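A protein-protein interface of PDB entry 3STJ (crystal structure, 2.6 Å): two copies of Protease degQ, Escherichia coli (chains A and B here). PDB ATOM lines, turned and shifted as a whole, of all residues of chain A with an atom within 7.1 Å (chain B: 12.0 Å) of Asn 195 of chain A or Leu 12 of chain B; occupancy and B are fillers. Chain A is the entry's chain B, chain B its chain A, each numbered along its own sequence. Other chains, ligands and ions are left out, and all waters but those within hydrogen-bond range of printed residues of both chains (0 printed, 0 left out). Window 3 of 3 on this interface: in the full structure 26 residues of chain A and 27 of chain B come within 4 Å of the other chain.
Printed residues of chain A that touch a printed residue of chain B: Arg 136, Asp 139, Phe 140, Leu 194 and Asn 195. Hydrophobic or aromatic side chains of chain B within 4 Å of the printed part of chain A: Leu 12, Pro 13, Leu 15 and Ala 16. Among the printed residues, 10 pairs touch across the chains. Among the printed residues, Asp or Glu carboxylates within 4 Å of a Lys or Arg side-chain nitrogen of the other chain: Arg 136 of chain A with Glu 20 of chain B.
Of chain B, only Leu 12 (3.5 Å) comes within 4 Å of Asn 195 of chain A. Printed residues of chain A within 4 Å of Leu 12 of chain B: Leu 194 (3.7 Å) and Asn 195 (3.5 Å). No residue of chain B comes within 4 Å of Met 18 of chain A. No residue of chain B comes within 4 Å of Ala 128 of chain A. No residue of chain B comes within 4 Å of Asn 193 of chain A. Of chain B, only Leu 12 (3.7 Å) and Pro 13 (3.6 Å) come within 4 Å of Leu 194 of chain A. Gly 196 of chain A touches none of the printed residues of chain B. No residue of chain B comes within 4 Å of Glu 197 of chain A. Of the printed residues of chain B, Phe 140 of chain A touches Pro 13 (3.3 Å), Ser 14 (3.7 Å) and Leu 15 (3.9 Å). Printed residues of chain A within 4 Å of Ser 14 of chain B: Asp 139 and Phe 140. Pro 11 of chain B touches none of the printed residues of chain A. The nearest residue of chain B that does not touch Asn 195 of chain A is Pro 11 of chain B (7.4 Å). The nearest printed residue of chain A that does not touch Ala 16 of chain B is Phe 140 of chain A (6.9 Å).
Among the printed residues, pairs that only touch across the chains: Phe 140 of chain A with Pro 13 of chain B (3.3 Å), Asn 195 of chain A with Leu 12 of chain B (3.5 Å), Arg 136 of chain A with Ala 16 of chain B (3.6 Å), Leu 194 of chain A with Pro 13 of chain B (3.6 Å), Phe 140 of chain A with Ser 14 of chain B (3.7 Å), Asp 139 of chain A with Ala 16 of chain B (3.7 Å), Leu 194 of chain A with Leu 12 of chain B (3.7 Å) and Phe 140 of chain A with Leu 15 of chain B (3.9 Å).
The side-chain hydroxyl of Ser 14 of chain B lies within hydrogen-bond range of the backbone NH of Ala 16 of chain B, at 3.0 Å. OD2 of Asp 139 of chain A is in hydrogen-bond range of N of Arg 136 of chain A (2.8 Å). OD1 of Asn 193 of chain A is in hydrogen-bond range of N of Asn 195 of chain A, 3.0 Å away.
The side-chain carboxylate of Asp 139 of chain A lies within hydrogen-bond range of the side-chain hydroxyl of Ser 14 of chain B, at 2.6 Å. The side-chain carboxylate (OE2) of Glu 20 of chain B is in salt-bridge range of the guanidinium group (NH1) of Arg 136 of chain A.
Position printed for both chains: 18. Of the 10 pairs that touch across the chains among the printed residues, none has its exchanged pair printed and touching as well.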
ATOM      1  N   MET A  18      34.794  15.646 -22.454  1.00  0.00           N
ATOM      2  CA  MET A  18      33.489  15.713 -21.769  1.00  0.00           C
ATOM      3  C   MET A  18      32.476  14.648 -22.274  1.00  0.00           C
ATOM      4  O   MET A  18      31.598  14.271 -21.499  1.00  0.00           O
ATOM      5  CB  MET A  18      32.849  17.117 -21.738  1.00  0.00           C
ATOM      6  CG  MET A  18      32.200  17.550 -23.005  1.00  0.00           C
ATOM      7  SD  MET A  18      30.425  17.185 -23.193  1.00  0.00           S
ATOM      8  CE  MET A  18      30.166  17.987 -24.820  1.00  0.00           C
ATOM      9  N   LYS A  21      32.519  11.137 -20.196  1.00  0.00           N
ATOM     10  CA  LYS A  21      31.878  11.112 -18.892  1.00  0.00           C
ATOM     11  C   LYS A  21      30.374  11.091 -18.942  1.00  0.00           C
ATOM     12  O   LYS A  21      29.728  10.566 -18.044  1.00  0.00           O
ATOM     13  CB  LYS A  21      32.291  12.358 -18.084  1.00  0.00           C
ATOM     14  CG  LYS A  21      33.762  12.737 -18.112  1.00  0.00           C
ATOM     15  CD  LYS A  21      33.989  13.951 -17.221  1.00  0.00           C
ATOM     16  CE  LYS A  21      35.281  14.660 -17.496  1.00  0.00           C
ATOM     17  NZ  LYS A  21      35.496  15.777 -16.544  1.00  0.00           N
ATOM     18  N   VAL A  22      29.815  11.715 -19.949  1.00  0.00           N
ATOM     19  CA  VAL A  22      28.385  12.021 -20.080  1.00  0.00           C
ATOM     20  C   VAL A  22      27.590  11.052 -21.000  1.00  0.00           C
ATOM     21  O   VAL A  22      26.444  10.755 -20.672  1.00  0.00           O
ATOM     22  CB  VAL A  22      28.388  13.484 -20.596  1.00  0.00           C
ATOM     23  CG1 VAL A  22      27.193  13.822 -21.460  1.00  0.00           C
ATOM     24  CG2 VAL A  22      28.577  14.464 -19.452  1.00  0.00           C
ATOM     25  N   ILE A 127      22.600  12.578 -15.905  1.00  0.00           N
ATOM     26  CA  ILE A 127      23.007  13.816 -16.530  1.00  0.00           C
ATOM     27  C   ILE A 127      22.805  14.991 -15.575  1.00  0.00           C
ATOM     28  O   ILE A 127      21.862  14.993 -14.767  1.00  0.00           O
ATOM     29  CB  ILE A 127      22.157  13.968 -17.843  1.00  0.00           C
ATOM     30  CG1 ILE A 127      22.985  13.979 -19.159  1.00  0.00           C
ATOM     31  CG2 ILE A 127      20.994  14.985 -17.790  1.00  0.00           C
ATOM     32  CD1 ILE A 127      24.066  14.796 -19.268  1.00  0.00           C
ATOM     33  N   ALA A 128      23.696  15.992 -15.691  1.00  0.00           N
ATOM     34  CA  ALA A 128      23.564  17.261 -14.991  1.00  0.00           C
ATOM     35  C   ALA A 128      22.677  18.146 -15.846  1.00  0.00           C
ATOM     36  O   ALA A 128      22.800  18.118 -17.071  1.00  0.00           O
ATOM     37  CB  ALA A 128      24.929  17.892 -14.780  1.00  0.00           C
ATOM     38  N   ARG A 136      22.095  31.242 -25.255  1.00  0.00           N
ATOM     39  CA  ARG A 136      22.142  32.301 -26.265  1.00  0.00           C
ATOM     40  C   ARG A 136      22.438  31.734 -27.622  1.00  0.00           C
ATOM     41  O   ARG A 136      23.112  30.696 -27.732  1.00  0.00           O
ATOM     42  CB  ARG A 136      23.198  33.350 -25.913  1.00  0.00           C
ATOM     43  CG  ARG A 136      22.751  34.344 -24.853  1.00  0.00           C
ATOM     44  CD  ARG A 136      23.818  35.380 -24.617  1.00  0.00           C
ATOM     45  NE  ARG A 136      25.092  34.763 -24.266  1.00  0.00           N
ATOM     46  CZ  ARG A 136      26.242  35.422 -24.250  1.00  0.00           C
ATOM     47  NH1 ARG A 136      26.277  36.718 -24.554  1.00  0.00           N
ATOM     48  NH2 ARG A 136      27.370  34.791 -23.945  1.00  0.00           N
ATOM     49  N   ASP A 139      25.785  29.654 -28.879  1.00  0.00           N
ATOM     50  CA  ASP A 139      26.291  28.660 -27.921  1.00  0.00           C
ATOM     51  C   ASP A 139      26.395  27.316 -28.612  1.00  0.00           C
ATOM     52  O   ASP A 139      25.561  26.988 -29.460  1.00  0.00           O
ATOM     53  CB  ASP A 139      25.410  28.567 -26.654  1.00  0.00           C
ATOM     54  CG  ASP A 139      25.442  29.777 -25.711  1.00  0.00           C
ATOM     55  OD1 ASP A 139      26.434  30.541 -25.742  1.00  0.00           O
ATOM     56  OD2 ASP A 139      24.495  29.933 -24.908  1.00  0.00           O
ATOM     57  N   PHE A 140      27.461  26.572 -28.324  1.00  0.00           N
ATOM     58  CA  PHE A 140      27.703  25.266 -28.949  1.00  0.00           C
ATOM     59  C   PHE A 140      26.853  24.198 -28.298  1.00  0.00           C
ATOM     60  O   PHE A 140      26.585  24.248 -27.100  1.00  0.00           O
ATOM     61  CB  PHE A 140      29.177  24.909 -28.905  1.00  0.00           C
ATOM     62  CG  PHE A 140      30.006  25.823 -29.768  1.00  0.00           C
ATOM     63  CD1 PHE A 140      30.800  26.813 -29.203  1.00  0.00           C
ATOM     64  CD2 PHE A 140      29.995  25.696 -31.156  1.00  0.00           C
ATOM     65  CE1 PHE A 140      31.588  27.655 -30.010  1.00  0.00           C
ATOM     66  CE2 PHE A 140      30.781  26.539 -31.962  1.00  0.00           C
ATOM     67  CZ  PHE A 140      31.565  27.519 -31.381  1.00  0.00           C
ATOM     68  N   LEU A 192      23.097  18.828 -25.409  1.00  0.00           N
ATOM     69  CA  LEU A 192      24.052  19.190 -24.355  1.00  0.00           C
ATOM     70  C   LEU A 192      24.872  20.426 -24.666  1.00  0.00           C
ATOM     71  O   LEU A 192      25.140  20.701 -25.836  1.00  0.00           O
ATOM     72  CB  LEU A 192      25.063  18.028 -24.119  1.00  0.00           C
ATOM     73  CG  LEU A 192      24.513  16.614 -24.002  1.00  0.00           C
ATOM     74  CD1 LEU A 192      25.607  15.631 -24.127  1.00  0.00           C
ATOM     75  CD2 LEU A 192      23.721  16.405 -22.717  1.00  0.00           C
ATOM     76  N   ASN A 193      25.390  21.079 -23.611  1.00  0.00           N
ATOM     77  CA  ASN A 193      26.330  22.171 -23.795  1.00  0.00           C
ATOM     78  C   ASN A 193      27.753  21.600 -23.783  1.00  0.00           C
ATOM     79  O   ASN A 193      27.924  20.376 -23.726  1.00  0.00           O
ATOM     80  CB  ASN A 193      26.123  23.277 -22.748  1.00  0.00           C
ATOM     81  CG  ASN A 193      26.284  22.879 -21.301  1.00  0.00           C
ATOM     82  OD1 ASN A 193      26.933  21.884 -20.952  1.00  0.00           O
ATOM     83  ND2 ASN A 193      25.704  23.690 -20.425  1.00  0.00           N
ATOM     84  N   LEU A 194      28.770  22.474 -23.826  1.00  0.00           N
ATOM     85  CA  LEU A 194      30.175  22.069 -23.832  1.00  0.00           C
ATOM     86  C   LEU A 194      30.661  21.524 -22.461  1.00  0.00           C
ATOM     87  O   LEU A 194      31.734  20.934 -22.415  1.00  0.00           O
ATOM     88  CB  LEU A 194      31.077  23.199 -24.328  1.00  0.00           C
ATOM     89  CG  LEU A 194      30.956  23.557 -25.813  1.00  0.00           C
ATOM     90  CD1 LEU A 194      31.898  24.654 -26.171  1.00  0.00           C
ATOM     91  CD2 LEU A 194      31.182  22.355 -26.710  1.00  0.00           C
ATOM     92  N   ASN A 195      29.856  21.633 -21.398  1.00  0.00           N
ATOM     93  CA  ASN A 195      30.153  21.044 -20.094  1.00  0.00           C
ATOM     94  C   ASN A 195      29.473  19.662 -19.947  1.00  0.00           C
ATOM     95  O   ASN A 195      29.595  19.020 -18.892  1.00  0.00           O
ATOM     96  CB  ASN A 195      29.668  21.960 -18.966  1.00  0.00           C
ATOM     97  CG  ASN A 195      30.506  23.178 -18.733  1.00  0.00           C
ATOM     98  OD1 ASN A 195      31.738  23.152 -18.831  1.00  0.00           O
ATOM     99  ND2 ASN A 195      29.845  24.268 -18.365  1.00  0.00           N
ATOM    100  N   GLY A 196      28.729  19.252 -20.980  1.00  0.00           N
ATOM    101  CA  GLY A 196      28.006  17.986 -20.995  1.00  0.00           C
ATOM    102  C   GLY A 196      26.758  18.012 -20.167  1.00  0.00           C
ATOM    103  O   GLY A 196      26.284  16.970 -19.722  1.00  0.00           O
ATOM    104  N   GLU A 197      26.223  19.207 -19.939  1.00  0.00           N
ATOM    105  CA  GLU A 197      24.997  19.411 -19.165  1.00  0.00           C
ATOM    106  C   GLU A 197      23.833  19.484 -20.127  1.00  0.00           C
ATOM    107  O   GLU A 197      23.967  20.028 -21.228  1.00  0.00           O
ATOM    108  CB  GLU A 197      25.083  20.694 -18.314  1.00  0.00           C
ATOM    109  CG  GLU A 197      26.174  20.694 -17.257  1.00  0.00           C
ATOM    110  CD  GLU A 197      26.666  22.052 -16.778  1.00  0.00           C
ATOM    111  OE1 GLU A 197      27.493  22.069 -15.838  1.00  0.00           O
ATOM    112  OE2 GLU A 197      26.251  23.092 -17.343  1.00  0.00           O
ATOM    113  N   LEU A 198      22.684  18.962 -19.703  1.00  0.00           N
ATOM    114  CA  LEU A 198      21.469  18.945 -20.512  1.00  0.00           C
ATOM    115  C   LEU A 198      20.912  20.347 -20.689  1.00  0.00           C
ATOM    116  O   LEU A 198      20.670  21.037 -19.703  1.00  0.00           O
ATOM    117  CB  LEU A 198      20.413  18.023 -19.876  1.00  0.00           C
ATOM    118  CG  LEU A 198      19.233  17.618 -20.748  1.00  0.00           C
ATOM    119  CD1 LEU A 198      19.645  16.587 -21.740  1.00  0.00           C
ATOM    120  CD2 LEU A 198      18.068  17.112 -19.907  1.00  0.00           C
ATOM    121  N   PRO B  11      33.274  31.613 -19.589  1.00  0.00           N
ATOM    122  CA  PRO B  11      34.492  30.806 -19.775  1.00  0.00           C
ATOM    123  C   PRO B  11      34.364  29.801 -20.926  1.00  0.00           C
ATOM    124  O   PRO B  11      35.383  29.478 -21.552  1.00  0.00           O
ATOM    125  CB  PRO B  11      34.664  30.089 -18.429  1.00  0.00           C
ATOM    126  CG  PRO B  11      33.922  30.940 -17.424  1.00  0.00           C
ATOM    127  CD  PRO B  11      32.991  31.879 -18.162  1.00  0.00           C
ATOM    128  N   LEU B  12      33.127  29.299 -21.203  1.00  0.00           N
ATOM    129  CA  LEU B  12      32.901  28.343 -22.289  1.00  0.00           C
ATOM    130  C   LEU B  12      32.952  29.037 -23.645  1.00  0.00           C
ATOM    131  O   LEU B  12      32.342  30.095 -23.794  1.00  0.00           O
ATOM    132  CB  LEU B  12      31.554  27.604 -22.142  1.00  0.00           C
ATOM    133  CG  LEU B  12      31.475  26.307 -21.313  1.00  0.00           C
ATOM    134  CD1 LEU B  12      30.143  25.609 -21.555  1.00  0.00           C
ATOM    135  CD2 LEU B  12      32.599  25.314 -21.648  1.00  0.00           C
ATOM    136  N   PRO B  13      33.639  28.445 -24.653  1.00  0.00           N
ATOM    137  CA  PRO B  13      33.637  29.058 -25.998  1.00  0.00           C
ATOM    138  C   PRO B  13      32.215  29.133 -26.567  1.00  0.00           C
ATOM    139  O   PRO B  13      31.394  28.238 -26.333  1.00  0.00           O
ATOM    140  CB  PRO B  13      34.531  28.131 -26.831  1.00  0.00           C
ATOM    141  CG  PRO B  13      35.175  27.212 -25.874  1.00  0.00           C
ATOM    142  CD  PRO B  13      34.372  27.162 -24.642  1.00  0.00           C
ATOM    143  N   SER B  14      31.923  30.225 -27.288  1.00  0.00           N
ATOM    144  CA  SER B  14      30.612  30.520 -27.846  1.00  0.00           C
ATOM    145  C   SER B  14      30.685  31.559 -28.937  1.00  0.00           C
ATOM    146  O   SER B  14      31.573  32.422 -28.893  1.00  0.00           O
ATOM    147  CB  SER B  14      29.693  31.042 -26.748  1.00  0.00           C
ATOM    148  OG  SER B  14      28.414  31.321 -27.290  1.00  0.00           O
ATOM    149  N   LEU B  15      29.698  31.527 -29.881  1.00  0.00           N
ATOM    150  CA  LEU B  15      29.579  32.518 -30.958  1.00  0.00           C
ATOM    151  C   LEU B  15      28.632  33.642 -30.541  1.00  0.00           C
ATOM    152  O   LEU B  15      28.536  34.662 -31.236  1.00  0.00           O
ATOM    153  CB  LEU B  15      29.102  31.879 -32.258  1.00  0.00           C
ATOM    154  CG  LEU B  15      29.987  30.806 -32.858  1.00  0.00           C
ATOM    155  CD1 LEU B  15      29.427  30.338 -34.172  1.00  0.00           C
ATOM    156  CD2 LEU B  15      31.458  31.261 -32.992  1.00  0.00           C
ATOM    157  N   ALA B  16      27.965  33.465 -29.379  1.00  0.00           N
ATOM    158  CA  ALA B  16      26.985  34.384 -28.805  1.00  0.00           C
ATOM    159  C   ALA B  16      27.553  35.788 -28.570  1.00  0.00           C
ATOM    160  O   ALA B  16      26.879  36.735 -28.974  1.00  0.00           O
ATOM    161  CB  ALA B  16      26.388  33.813 -27.524  1.00  0.00           C
ATOM    162  N   PRO B  17      28.769  35.998 -27.984  1.00  0.00           N
ATOM    163  CA  PRO B  17      29.246  37.393 -27.801  1.00  0.00           C
ATOM    164  C   PRO B  17      29.312  38.176 -29.129  1.00  0.00           C
ATOM    165  O   PRO B  17      28.849  39.314 -29.158  1.00  0.00           O
ATOM    166  CB  PRO B  17      30.613  37.215 -27.153  1.00  0.00           C
ATOM    167  CG  PRO B  17      30.530  35.875 -26.479  1.00  0.00           C
ATOM    168  CD  PRO B  17      29.738  35.032 -27.404  1.00  0.00           C
ATOM    169  N   MET B  18      29.775  37.558 -30.239  1.00  0.00           N
ATOM    170  CA  MET B  18      29.806  38.289 -31.506  1.00  0.00           C
ATOM    171  C   MET B  18      28.408  38.353 -32.169  1.00  0.00           C
ATOM    172  O   MET B  18      28.079  39.375 -32.768  1.00  0.00           O
ATOM    173  CB  MET B  18      30.903  37.780 -32.478  1.00  0.00           C
ATOM    174  CG  MET B  18      30.524  36.632 -33.355  1.00  0.00           C
ATOM    175  SD  MET B  18      29.648  37.087 -34.880  1.00  0.00           S
ATOM    176  CE  MET B  18      29.616  35.478 -35.669  1.00  0.00           C
ATOM    177  N   LEU B  19      27.589  37.314 -32.048  1.00  0.00           N
ATOM    178  CA  LEU B  19      26.269  37.329 -32.676  1.00  0.00           C
ATOM    179  C   LEU B  19      25.318  38.363 -32.043  1.00  0.00           C
ATOM    180  O   LEU B  19      24.553  39.002 -32.768  1.00  0.00           O
ATOM    181  CB  LEU B  19      25.654  35.934 -32.667  1.00  0.00           C
ATOM    182  CG  LEU B  19      26.254  35.008 -33.736  1.00  0.00           C
ATOM    183  CD1 LEU B  19      25.909  33.592 -33.473  1.00  0.00           C
ATOM    184  CD2 LEU B  19      25.827  35.417 -35.142  1.00  0.00           C
ATOM    185  N   GLU B  20      25.453  38.590 -30.716  1.00  0.00           N
ATOM    186  CA  GLU B  20      24.685  39.557 -29.919  1.00  0.00           C
ATOM    187  C   GLU B  20      24.722  40.955 -30.552  1.00  0.00           C
ATOM    188  O   GLU B  20      23.690  41.619 -30.634  1.00  0.00           O
ATOM    189  CB  GLU B  20      25.308  39.626 -28.528  1.00  0.00           C
ATOM    190  CG  GLU B  20      24.369  39.490 -27.350  1.00  0.00           C
ATOM    191  CD  GLU B  20      25.080  39.292 -26.016  1.00  0.00           C
ATOM    192  OE1 GLU B  20      26.296  39.589 -25.919  1.00  0.00           O
ATOM    193  OE2 GLU B  20      24.423  38.798 -25.070  1.00  0.00           O
